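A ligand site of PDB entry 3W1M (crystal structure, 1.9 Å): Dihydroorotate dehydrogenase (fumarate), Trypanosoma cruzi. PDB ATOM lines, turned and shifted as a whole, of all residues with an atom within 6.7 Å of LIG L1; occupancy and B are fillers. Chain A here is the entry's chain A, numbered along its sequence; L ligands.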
ATOM      1  N   ALA A  20      -5.407 -16.359  17.958  1.00  0.00           N
ATOM      2  CA  ALA A  20      -5.143 -14.926  17.854  1.00  0.00           C
ATOM      3  C   ALA A  20      -4.999 -14.282  19.244  1.00  0.00           C
ATOM      4  O   ALA A  20      -5.732 -14.578  20.204  1.00  0.00           O
ATOM      5  CB  ALA A  20      -6.217 -14.172  17.042  1.00  0.00           C
ATOM      6  N   GLY A  21      -4.067 -13.360  19.289  1.00  0.00           N
ATOM      7  CA  GLY A  21      -3.746 -12.640  20.511  1.00  0.00           C
ATOM      8  C   GLY A  21      -2.653 -13.258  21.347  1.00  0.00           C
ATOM      9  O   GLY A  21      -2.064 -12.565  22.166  1.00  0.00           O
ATOM     10  N   LYS A  44      -2.060 -10.786  16.078  1.00  0.00           N
ATOM     11  CA  LYS A  44      -2.938 -10.189  17.064  1.00  0.00           C
ATOM     12  C   LYS A  44      -4.049  -9.378  16.401  1.00  0.00           C
ATOM     13  O   LYS A  44      -3.777  -8.628  15.473  1.00  0.00           O
ATOM     14  CB  LYS A  44      -2.114  -9.255  17.993  1.00  0.00           C
ATOM     15  CG  LYS A  44      -2.951  -8.300  18.840  1.00  0.00           C
ATOM     16  CD  LYS A  44      -3.577  -9.060  20.025  1.00  0.00           C
ATOM     17  CE  LYS A  44      -4.637  -8.267  20.753  1.00  0.00           C
ATOM     18  NZ  LYS A  44      -5.344  -9.106  21.783  1.00  0.00           N
ATOM     19  N   SER A  45      -5.265  -9.438  16.928  1.00  0.00           N
ATOM     20  CA  SER A  45      -6.356  -8.686  16.352  1.00  0.00           C
ATOM     21  C   SER A  45      -5.947  -7.221  16.368  1.00  0.00           C
ATOM     22  O   SER A  45      -5.473  -6.743  17.384  1.00  0.00           O
ATOM     23  CB  SER A  45      -7.702  -8.821  17.047  1.00  0.00           C
ATOM     24  OG  SER A  45      -8.260 -10.079  16.761  1.00  0.00           O
ATOM     25  N   ASN A  54      -6.083  -2.257  27.881  1.00  0.00           N
ATOM     26  CA  ASN A  54      -6.594  -2.017  29.223  1.00  0.00           C
ATOM     27  C   ASN A  54      -5.495  -1.935  30.293  1.00  0.00           C
ATOM     28  O   ASN A  54      -4.336  -2.361  30.125  1.00  0.00           O
ATOM     29  CB  ASN A  54      -7.680  -3.100  29.583  1.00  0.00           C
ATOM     30  CG  ASN A  54      -8.963  -2.994  28.779  1.00  0.00           C
ATOM     31  OD1 ASN A  54      -9.333  -1.937  28.176  1.00  0.00           O
ATOM     32  ND2 ASN A  54      -9.737  -4.082  28.820  1.00  0.00           N
ATOM     33  N   ASN A  68      -8.890 -13.037  30.737  1.00  0.00           N
ATOM     34  CA  ASN A  68      -8.171 -11.862  30.211  1.00  0.00           C
ATOM     35  C   ASN A  68      -9.125 -10.763  29.848  1.00  0.00           C
ATOM     36  O   ASN A  68     -10.228 -11.022  29.402  1.00  0.00           O
ATOM     37  CB  ASN A  68      -7.270 -12.147  28.997  1.00  0.00           C
ATOM     38  CG  ASN A  68      -8.034 -12.154  27.687  1.00  0.00           C
ATOM     39  OD1 ASN A  68      -8.291 -11.067  27.048  1.00  0.00           O
ATOM     40  ND2 ASN A  68      -8.550 -13.300  27.328  1.00  0.00           N
ATOM     41  N   SER A  69      -8.720  -9.511  30.094  1.00  0.00           N
ATOM     42  CA  SER A  69      -9.427  -8.394  29.465  1.00  0.00           C
ATOM     43  C   SER A  69      -8.334  -7.467  28.891  1.00  0.00           C
ATOM     44  O   SER A  69      -8.024  -6.352  29.447  1.00  0.00           O
ATOM     45  CB  SER A  69     -10.261  -7.646  30.519  1.00  0.00           C
ATOM     46  OG  SER A  69     -10.829  -6.478  29.979  1.00  0.00           O
ATOM     47  N   MET A  70      -7.662  -7.991  27.860  1.00  0.00           N
ATOM     48  CA  MET A  70      -6.463  -7.278  27.407  1.00  0.00           C
ATOM     49  C   MET A  70      -6.857  -5.855  26.896  1.00  0.00           C
ATOM     50  O   MET A  70      -6.115  -4.895  27.054  1.00  0.00           O
ATOM     51  CB  MET A  70      -5.730  -7.996  26.282  1.00  0.00           C
ATOM     52  CG  MET A  70      -5.348  -9.419  26.554  1.00  0.00           C
ATOM     53  SD  MET A  70      -4.263  -9.629  27.978  1.00  0.00           S
ATOM     54  CE  MET A  70      -2.743  -8.976  27.356  1.00  0.00           C
ATOM     55  N   GLY A  71      -7.971  -5.798  26.192  1.00  0.00           N
ATOM     56  CA  GLY A  71      -8.516  -4.569  25.610  1.00  0.00           C
ATOM     57  C   GLY A  71      -7.946  -4.222  24.250  1.00  0.00           C
ATOM     58  O   GLY A  71      -7.843  -3.053  23.916  1.00  0.00           O
ATOM     59  N   LEU A  72      -7.603  -5.257  23.495  1.00  0.00           N
ATOM     60  CA  LEU A  72      -7.170  -5.132  22.114  1.00  0.00           C
ATOM     61  C   LEU A  72      -5.939  -4.239  21.992  1.00  0.00           C
ATOM     62  O   LEU A  72      -5.821  -3.374  21.112  1.00  0.00           O
ATOM     63  CB  LEU A  72      -8.345  -4.555  21.342  1.00  0.00           C
ATOM     64  CG  LEU A  72      -8.529  -4.591  19.831  1.00  0.00           C
ATOM     65  CD1 LEU A  72      -8.103  -5.943  19.254  1.00  0.00           C
ATOM     66  CD2 LEU A  72     -10.032  -4.322  19.493  1.00  0.00           C
ATOM     67  N   PRO A  73      -4.993  -4.456  22.860  1.00  0.00           N
ATOM     68  CA  PRO A  73      -3.714  -3.762  22.697  1.00  0.00           C
ATOM     69  C   PRO A  73      -3.039  -4.310  21.419  1.00  0.00           C
ATOM     70  O   PRO A  73      -2.969  -5.527  21.238  1.00  0.00           O
ATOM     71  CB  PRO A  73      -2.872  -4.248  23.867  1.00  0.00           C
ATOM     72  CG  PRO A  73      -3.477  -5.587  24.223  1.00  0.00           C
ATOM     73  CD  PRO A  73      -4.956  -5.417  23.964  1.00  0.00           C
ATOM     74  N   SER A 100      -9.828  -6.561  13.937  1.00  0.00           N
ATOM     75  CA  SER A 100     -10.852  -6.357  14.929  1.00  0.00           C
ATOM     76  C   SER A 100     -11.192  -4.868  15.087  1.00  0.00           C
ATOM     77  O   SER A 100     -11.191  -4.334  16.173  1.00  0.00           O
ATOM     78  CB  SER A 100     -10.403  -7.005  16.244  1.00  0.00           C
ATOM     79  OG  SER A 100     -11.500  -7.061  17.050  1.00  0.00           O
ATOM     80  N   ASN A 128     -12.552 -10.711  13.222  1.00  0.00           N
ATOM     81  CA  ASN A 128     -12.946 -10.967  14.606  1.00  0.00           C
ATOM     82  C   ASN A 128     -14.263 -10.332  14.989  1.00  0.00           C
ATOM     83  O   ASN A 128     -14.323  -9.161  15.167  1.00  0.00           O
ATOM     84  CB  ASN A 128     -11.862 -10.449  15.554  1.00  0.00           C
ATOM     85  CG  ASN A 128     -12.110 -10.772  17.009  1.00  0.00           C
ATOM     86  OD1 ASN A 128     -13.085 -11.386  17.391  1.00  0.00           O
ATOM     87  ND2 ASN A 128     -11.184 -10.363  17.830  1.00  0.00           N
ATOM     88  N   SER A 130     -15.965 -11.235  17.867  1.00  0.00           N
ATOM     89  CA  SER A 130     -16.171 -11.794  19.151  1.00  0.00           C
ATOM     90  C   SER A 130     -15.307 -11.275  20.348  1.00  0.00           C
ATOM     91  O   SER A 130     -15.172 -11.922  21.308  1.00  0.00           O
ATOM     92  CB  SER A 130     -16.139 -13.315  19.047  1.00  0.00           C
ATOM     93  OG  SER A 130     -15.057 -13.697  18.339  1.00  0.00           O
ATOM     94  N   CYS A 131     -14.794 -10.094  20.217  1.00  0.00           N
ATOM     95  CA  CYS A 131     -14.025  -9.496  21.330  1.00  0.00           C
ATOM     96  C   CYS A 131     -14.968  -9.200  22.473  1.00  0.00           C
ATOM     97  O   CYS A 131     -15.796  -8.376  22.319  1.00  0.00           O
ATOM     98  CB  CYS A 131     -13.448  -8.169  20.917  1.00  0.00           C
ATOM     99  SG  CYS A 131     -12.390  -7.595  22.275  1.00  0.00           S
ATOM    100  N   PRO A 132     -14.769  -9.835  23.636  1.00  0.00           N
ATOM    101  CA  PRO A 132     -15.721  -9.630  24.733  1.00  0.00           C
ATOM    102  C   PRO A 132     -15.190  -8.592  25.784  1.00  0.00           C
ATOM    103  O   PRO A 132     -15.837  -8.469  26.863  1.00  0.00           O
ATOM    104  CB  PRO A 132     -15.784 -11.027  25.379  1.00  0.00           C
ATOM    105  CG  PRO A 132     -14.292 -11.475  25.303  1.00  0.00           C
ATOM    106  CD  PRO A 132     -13.729 -10.789  24.041  1.00  0.00           C
ATOM    107  N   ASN A 133     -14.082  -7.833  25.481  1.00  0.00           N
ATOM    108  CA  ASN A 133     -13.307  -7.021  26.540  1.00  0.00           C
ATOM    109  C   ASN A 133     -13.165  -5.489  26.367  1.00  0.00           C
ATOM    110  O   ASN A 133     -12.354  -4.846  27.079  1.00  0.00           O
ATOM    111  CB  ASN A 133     -11.895  -7.572  26.655  1.00  0.00           C
ATOM    112  CG  ASN A 133     -11.913  -8.983  27.188  1.00  0.00           C
ATOM    113  OD1 ASN A 133     -12.764  -9.285  28.079  1.00  0.00           O
ATOM    114  ND2 ASN A 133     -10.998  -9.844  26.676  1.00  0.00           N
ATOM    115  N   VAL A 134     -13.826  -4.950  25.353  1.00  0.00           N
ATOM    116  CA  VAL A 134     -13.726  -3.495  25.113  1.00  0.00           C
ATOM    117  C   VAL A 134     -15.037  -2.877  25.667  1.00  0.00           C
ATOM    118  O   VAL A 134     -16.097  -3.257  25.211  1.00  0.00           O
ATOM    119  CB  VAL A 134     -13.423  -3.163  23.636  1.00  0.00           C
ATOM    120  CG1 VAL A 134     -13.505  -1.632  23.421  1.00  0.00           C
ATOM    121  CG2 VAL A 134     -12.003  -3.649  23.257  1.00  0.00           C
ATOM    122  N   LYS A 165     -13.927 -15.218  13.307  1.00  0.00           N
ATOM    123  CA  LYS A 165     -13.705 -15.682  14.683  1.00  0.00           C
ATOM    124  C   LYS A 165     -14.991 -15.466  15.482  1.00  0.00           C
ATOM    125  O   LYS A 165     -15.422 -14.298  15.650  1.00  0.00           O
ATOM    126  CB  LYS A 165     -12.562 -14.935  15.307  1.00  0.00           C
ATOM    127  CG  LYS A 165     -12.234 -15.434  16.724  1.00  0.00           C
ATOM    128  CD  LYS A 165     -11.568 -16.806  16.738  1.00  0.00           C
ATOM    129  CE  LYS A 165     -10.894 -17.163  18.108  1.00  0.00           C
ATOM    130  NZ  LYS A 165      -9.764 -16.311  18.448  1.00  0.00           N
ATOM    131  N   ASN A 195     -13.791 -18.010  20.289  1.00  0.00           N
ATOM    132  CA  ASN A 195     -13.238 -16.965  21.162  1.00  0.00           C
ATOM    133  C   ASN A 195     -13.502 -17.311  22.594  1.00  0.00           C
ATOM    134  O   ASN A 195     -14.194 -18.315  22.893  1.00  0.00           O
ATOM    135  CB  ASN A 195     -13.785 -15.584  20.786  1.00  0.00           C
ATOM    136  CG  ASN A 195     -12.766 -14.449  21.004  1.00  0.00           C
ATOM    137  OD1 ASN A 195     -12.041 -14.329  22.014  1.00  0.00           O
ATOM    138  ND2 ASN A 195     -12.660 -13.630  19.993  1.00  0.00           N
ATOM    139  N   SER A 196     -12.958 -16.487  23.476  1.00  0.00           N
ATOM    140  CA  SER A 196     -13.075 -16.722  24.934  1.00  0.00           C
ATOM    141  C   SER A 196     -14.483 -16.690  25.358  1.00  0.00           C
ATOM    142  O   SER A 196     -15.388 -16.088  24.691  1.00  0.00           O
ATOM    143  CB  SER A 196     -12.118 -15.728  25.712  1.00  0.00           C
ATOM    144  OG  SER A 196     -12.461 -14.458  25.403  1.00  0.00           O
ATOM    145  N   VAL A 197     -14.771 -17.485  26.398  1.00  0.00           N
ATOM    146  CA  VAL A 197     -16.099 -17.489  27.013  1.00  0.00           C
ATOM    147  C   VAL A 197     -16.262 -16.180  27.829  1.00  0.00           C
ATOM    148  O   VAL A 197     -15.578 -15.938  28.826  1.00  0.00           O
ATOM    149  CB  VAL A 197     -16.305 -18.748  27.800  1.00  0.00           C
ATOM    150  CG1 VAL A 197     -17.562 -18.606  28.637  1.00  0.00           C
ATOM    151  CG2 VAL A 197     -16.351 -19.979  26.890  1.00  0.00           C
ATOM    152  N   GLY A 220     -12.655 -12.576  29.555  1.00  0.00           N
ATOM    153  CA  GLY A 220     -12.909 -13.795  28.793  1.00  0.00           C
ATOM    154  C   GLY A 220     -12.136 -14.971  29.369  1.00  0.00           C
ATOM    155  O   GLY A 220     -10.954 -14.845  29.746  1.00  0.00           O
ATOM    156  N   LEU A 221     -12.794 -16.123  29.406  1.00  0.00           N
ATOM    157  CA  LEU A 221     -12.186 -17.345  29.914  1.00  0.00           C
ATOM    158  C   LEU A 221     -11.697 -18.202  28.781  1.00  0.00           C
ATOM    159  O   LEU A 221     -12.361 -18.366  27.722  1.00  0.00           O
ATOM    160  CB  LEU A 221     -13.187 -18.154  30.671  1.00  0.00           C
ATOM    161  CG  LEU A 221     -13.934 -17.428  31.822  1.00  0.00           C
ATOM    162  CD1 LEU A 221     -15.105 -18.291  32.313  1.00  0.00           C
ATOM    163  CD2 LEU A 221     -12.984 -17.133  32.923  1.00  0.00           C
HETATM  164  O1  LIG L   1      -8.866  -8.377  24.985  1.00  0.00           O
HETATM  165  C1  LIG L   1      -8.360  -8.831  23.871  1.00  0.00           C
HETATM  166  O2  LIG L   1      -7.566  -8.125  23.253  1.00  0.00           O
HETATM  167  C2  LIG L   1      -9.002  -9.972  23.367  1.00  0.00           C
HETATM  168  C3  LIG L   1      -9.662 -10.013  22.120  1.00  0.00           C
HETATM  169 BR1  LIG L   1      -9.370  -8.675  20.852  1.00  0.00          BR
HETATM  170  C4  LIG L   1     -10.412 -11.128  21.728  1.00  0.00           C
HETATM  171  O3  LIG L   1     -11.016 -11.199  20.669  1.00  0.00           O
HETATM  172  N1  LIG L   1     -10.553 -12.168  22.663  1.00  0.00           N
HETATM  173  C5  LIG L   1      -9.994 -12.101  23.933  1.00  0.00           C
HETATM  174  O4  LIG L   1     -10.146 -13.048  24.729  1.00  0.00           O
HETATM  175  N2  LIG L   1      -9.227 -10.995  24.255  1.00  0.00           N
HETATM  176  N1  LG2 L   2      -8.923 -13.756  20.253  1.00  0.00           N
HETATM  177  C1  LG2 L   2      -8.954 -12.987  19.131  1.00  0.00           C
HETATM  178  O1  LG2 L   2      -9.684 -13.359  18.152  1.00  0.00           O
HETATM  179  N2  LG2 L   2      -8.151 -11.902  18.990  1.00  0.00           N
HETATM  180  C2  LG2 L   2      -7.289 -11.501  19.886  1.00  0.00           C
HETATM  181  O2  LG2 L   2      -6.520 -10.493  19.764  1.00  0.00           O
HETATM  182  C3  LG2 L   2      -7.230 -12.249  21.131  1.00  0.00           C
HETATM  183  N3  LG2 L   2      -6.348 -11.941  22.079  1.00  0.00           N
HETATM  184  C4  LG2 L   2      -6.199 -12.784  23.143  1.00  0.00           C
HETATM  185  C5  LG2 L   2      -5.335 -12.468  24.161  1.00  0.00           C
HETATM  186  C6  LG2 L   2      -5.154 -13.298  25.237  1.00  0.00           C
HETATM  187  C7  LG2 L   2      -4.102 -12.964  26.284  1.00  0.00           C
HETATM  188  C8  LG2 L   2      -5.959 -14.530  25.342  1.00  0.00           C
HETATM  189  C9  LG2 L   2      -5.797 -15.466  26.524  1.00  0.00           C
HETATM  190  C10 LG2 L   2      -6.894 -14.858  24.363  1.00  0.00           C
HETATM  191  C11 LG2 L   2      -7.089 -13.979  23.299  1.00  0.00           C
HETATM  192  N4  LG2 L   2      -8.021 -14.259  22.329  1.00  0.00           N
HETATM  193  C12 LG2 L   2      -8.079 -13.472  21.224  1.00  0.00           C
HETATM  194  C13 LG2 L   2      -8.826 -15.464  22.404  1.00  0.00           C
HETATM  195  C14 LG2 L   2      -8.059 -16.656  21.946  1.00  0.00           C
HETATM  196  O3  LG2 L   2      -7.774 -16.492  20.548  1.00  0.00           O
HETATM  197  C15 LG2 L   2      -8.935 -17.895  22.019  1.00  0.00           C
HETATM  198  O4  LG2 L   2     -10.091 -17.807  21.168  1.00  0.00           O
HETATM  199  C16 LG2 L   2      -9.371 -18.198  23.467  1.00  0.00           C
HETATM  200  O5  LG2 L   2      -8.296 -17.846  24.346  1.00  0.00           O
HETATM  201  C17 LG2 L   2      -9.771 -19.638  23.703  1.00  0.00           C
HETATM  202  O6  LG2 L   2      -8.732 -20.583  23.430  1.00  0.00           O
HETATM  203  P1  LG2 L   2      -7.851 -21.251  24.608  1.00  0.00           P
HETATM  204  O7  LG2 L   2      -6.818 -22.110  23.864  1.00  0.00           O
HETATM  205  O8  LG2 L   2      -8.802 -22.101  25.414  1.00  0.00           O
HETATM  206  O9  LG2 L   2      -7.237 -20.097  25.419  1.00  0.00           O
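N1 of LIG L1 is in hydrogen-bond range of OD1 of Asn 195, at 2.7 Å. An oxygen (O4) of LIG L1 lies within hydrogen-bond range of the side-chain hydroxyl (OG) of Ser 196 (2.8 Å). NZ of Lys 44 is in salt-bridge range of O2 of LIG L1, 2.8 Å away. The backbone NH of Leu 72 lies within hydrogen-bond range of an oxygen (O2) of LIG L1 (2.9 Å). OD1 of Asn 68 sits at hydrogen-bond distance from N2 of LIG L1 (2.9 Å). O3 of LIG L1 sits at hydrogen-bond distance from ND2 of Asn 128, at 3.0 Å. N of Gly 71 lies within hydrogen-bond range of O1 of LIG L1. An oxygen (O1) of LIG L1 lies within hydrogen-bond range of the side-chain amide nitrogen of Asn 133. An oxygen (O1) of LIG L1 lies within hydrogen-bond range of the backbone NH of Met 70, at 3.1 Å. NZ of Lys 44 lies within hydrogen-bond range of O2 of LG2 L2, at 2.7 Å. ND2 of Asn 128 lies within hydrogen-bond range of O1 of LG2 L2. The backbone NH of Ser 45 lies within hydrogen-bond range of an oxygen (O2) of LG2 L2, at 3.3 Å. A nitrogen (N2) of LG2 L2 is in hydrogen-bond range of the side-chain hydroxyl (OG) of Ser 45, 2.9 Å away. NZ of Lys 165 lies within hydrogen-bond range of O3 of LG2 L2, at 2.9 Å. O of Ala 20 lies close to O3 of LG2 L2 (2.8 Å).
OG of Ser 196 is in hydrogen-bond range of OD1 of Asn 195, at 3.4 Å. OD1 of Asn 128 is in hydrogen-bond range of ND2 of Asn 195 (3.5 Å). ND2 of Asn 133 is in hydrogen-bond range of OD1 of Asn 68. OD1 of Asn 68 is in hydrogen-bond range of N of Met 70 (3.2 Å). The side-chain hydroxyl (OG) of Ser 45 sits at hydrogen-bond distance from the side-chain amide nitrogen (ND2) of Asn 128, at 3.1 Å. The side-chain amide nitrogen of Asn 128 lies within hydrogen-bond range of the side-chain hydroxyl of Ser 100 (3.4 Å). The backbone carbonyl oxygen (O) of Asn 133 sits at hydrogen-bond distance from the side-chain amide nitrogen (ND2) of Asn 54, at 3.2 Å. The backbone NH (N) of Asn 54 is in hydrogen-bond range of the backbone carbonyl oxygen (O) of Met 70.
CD of Pro 73 touches O2 of LIG L1 (3.8 Å). SG of Cys 131 touches BR1 of LIG L1, 3.5 Å away. CD of Pro 132 touches N1 of LIG L1 (3.7 Å). Hydrophobic or aromatic side chains that line LIG L1: Met 70, Leu 72, Pro 73 and Pro 132. Within 4 Å of LIG L1: Lys 44, Asn 68, Met 70, Gly 71, Leu 72, Pro 73, Asn 128, Cys 131, Pro 132, Asn 133, Asn 195 and Ser 196.
A nitrogen (N1) of LG2 L2 sits close to a nitrogen (N1) of LIG L1 (3.3 Å).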
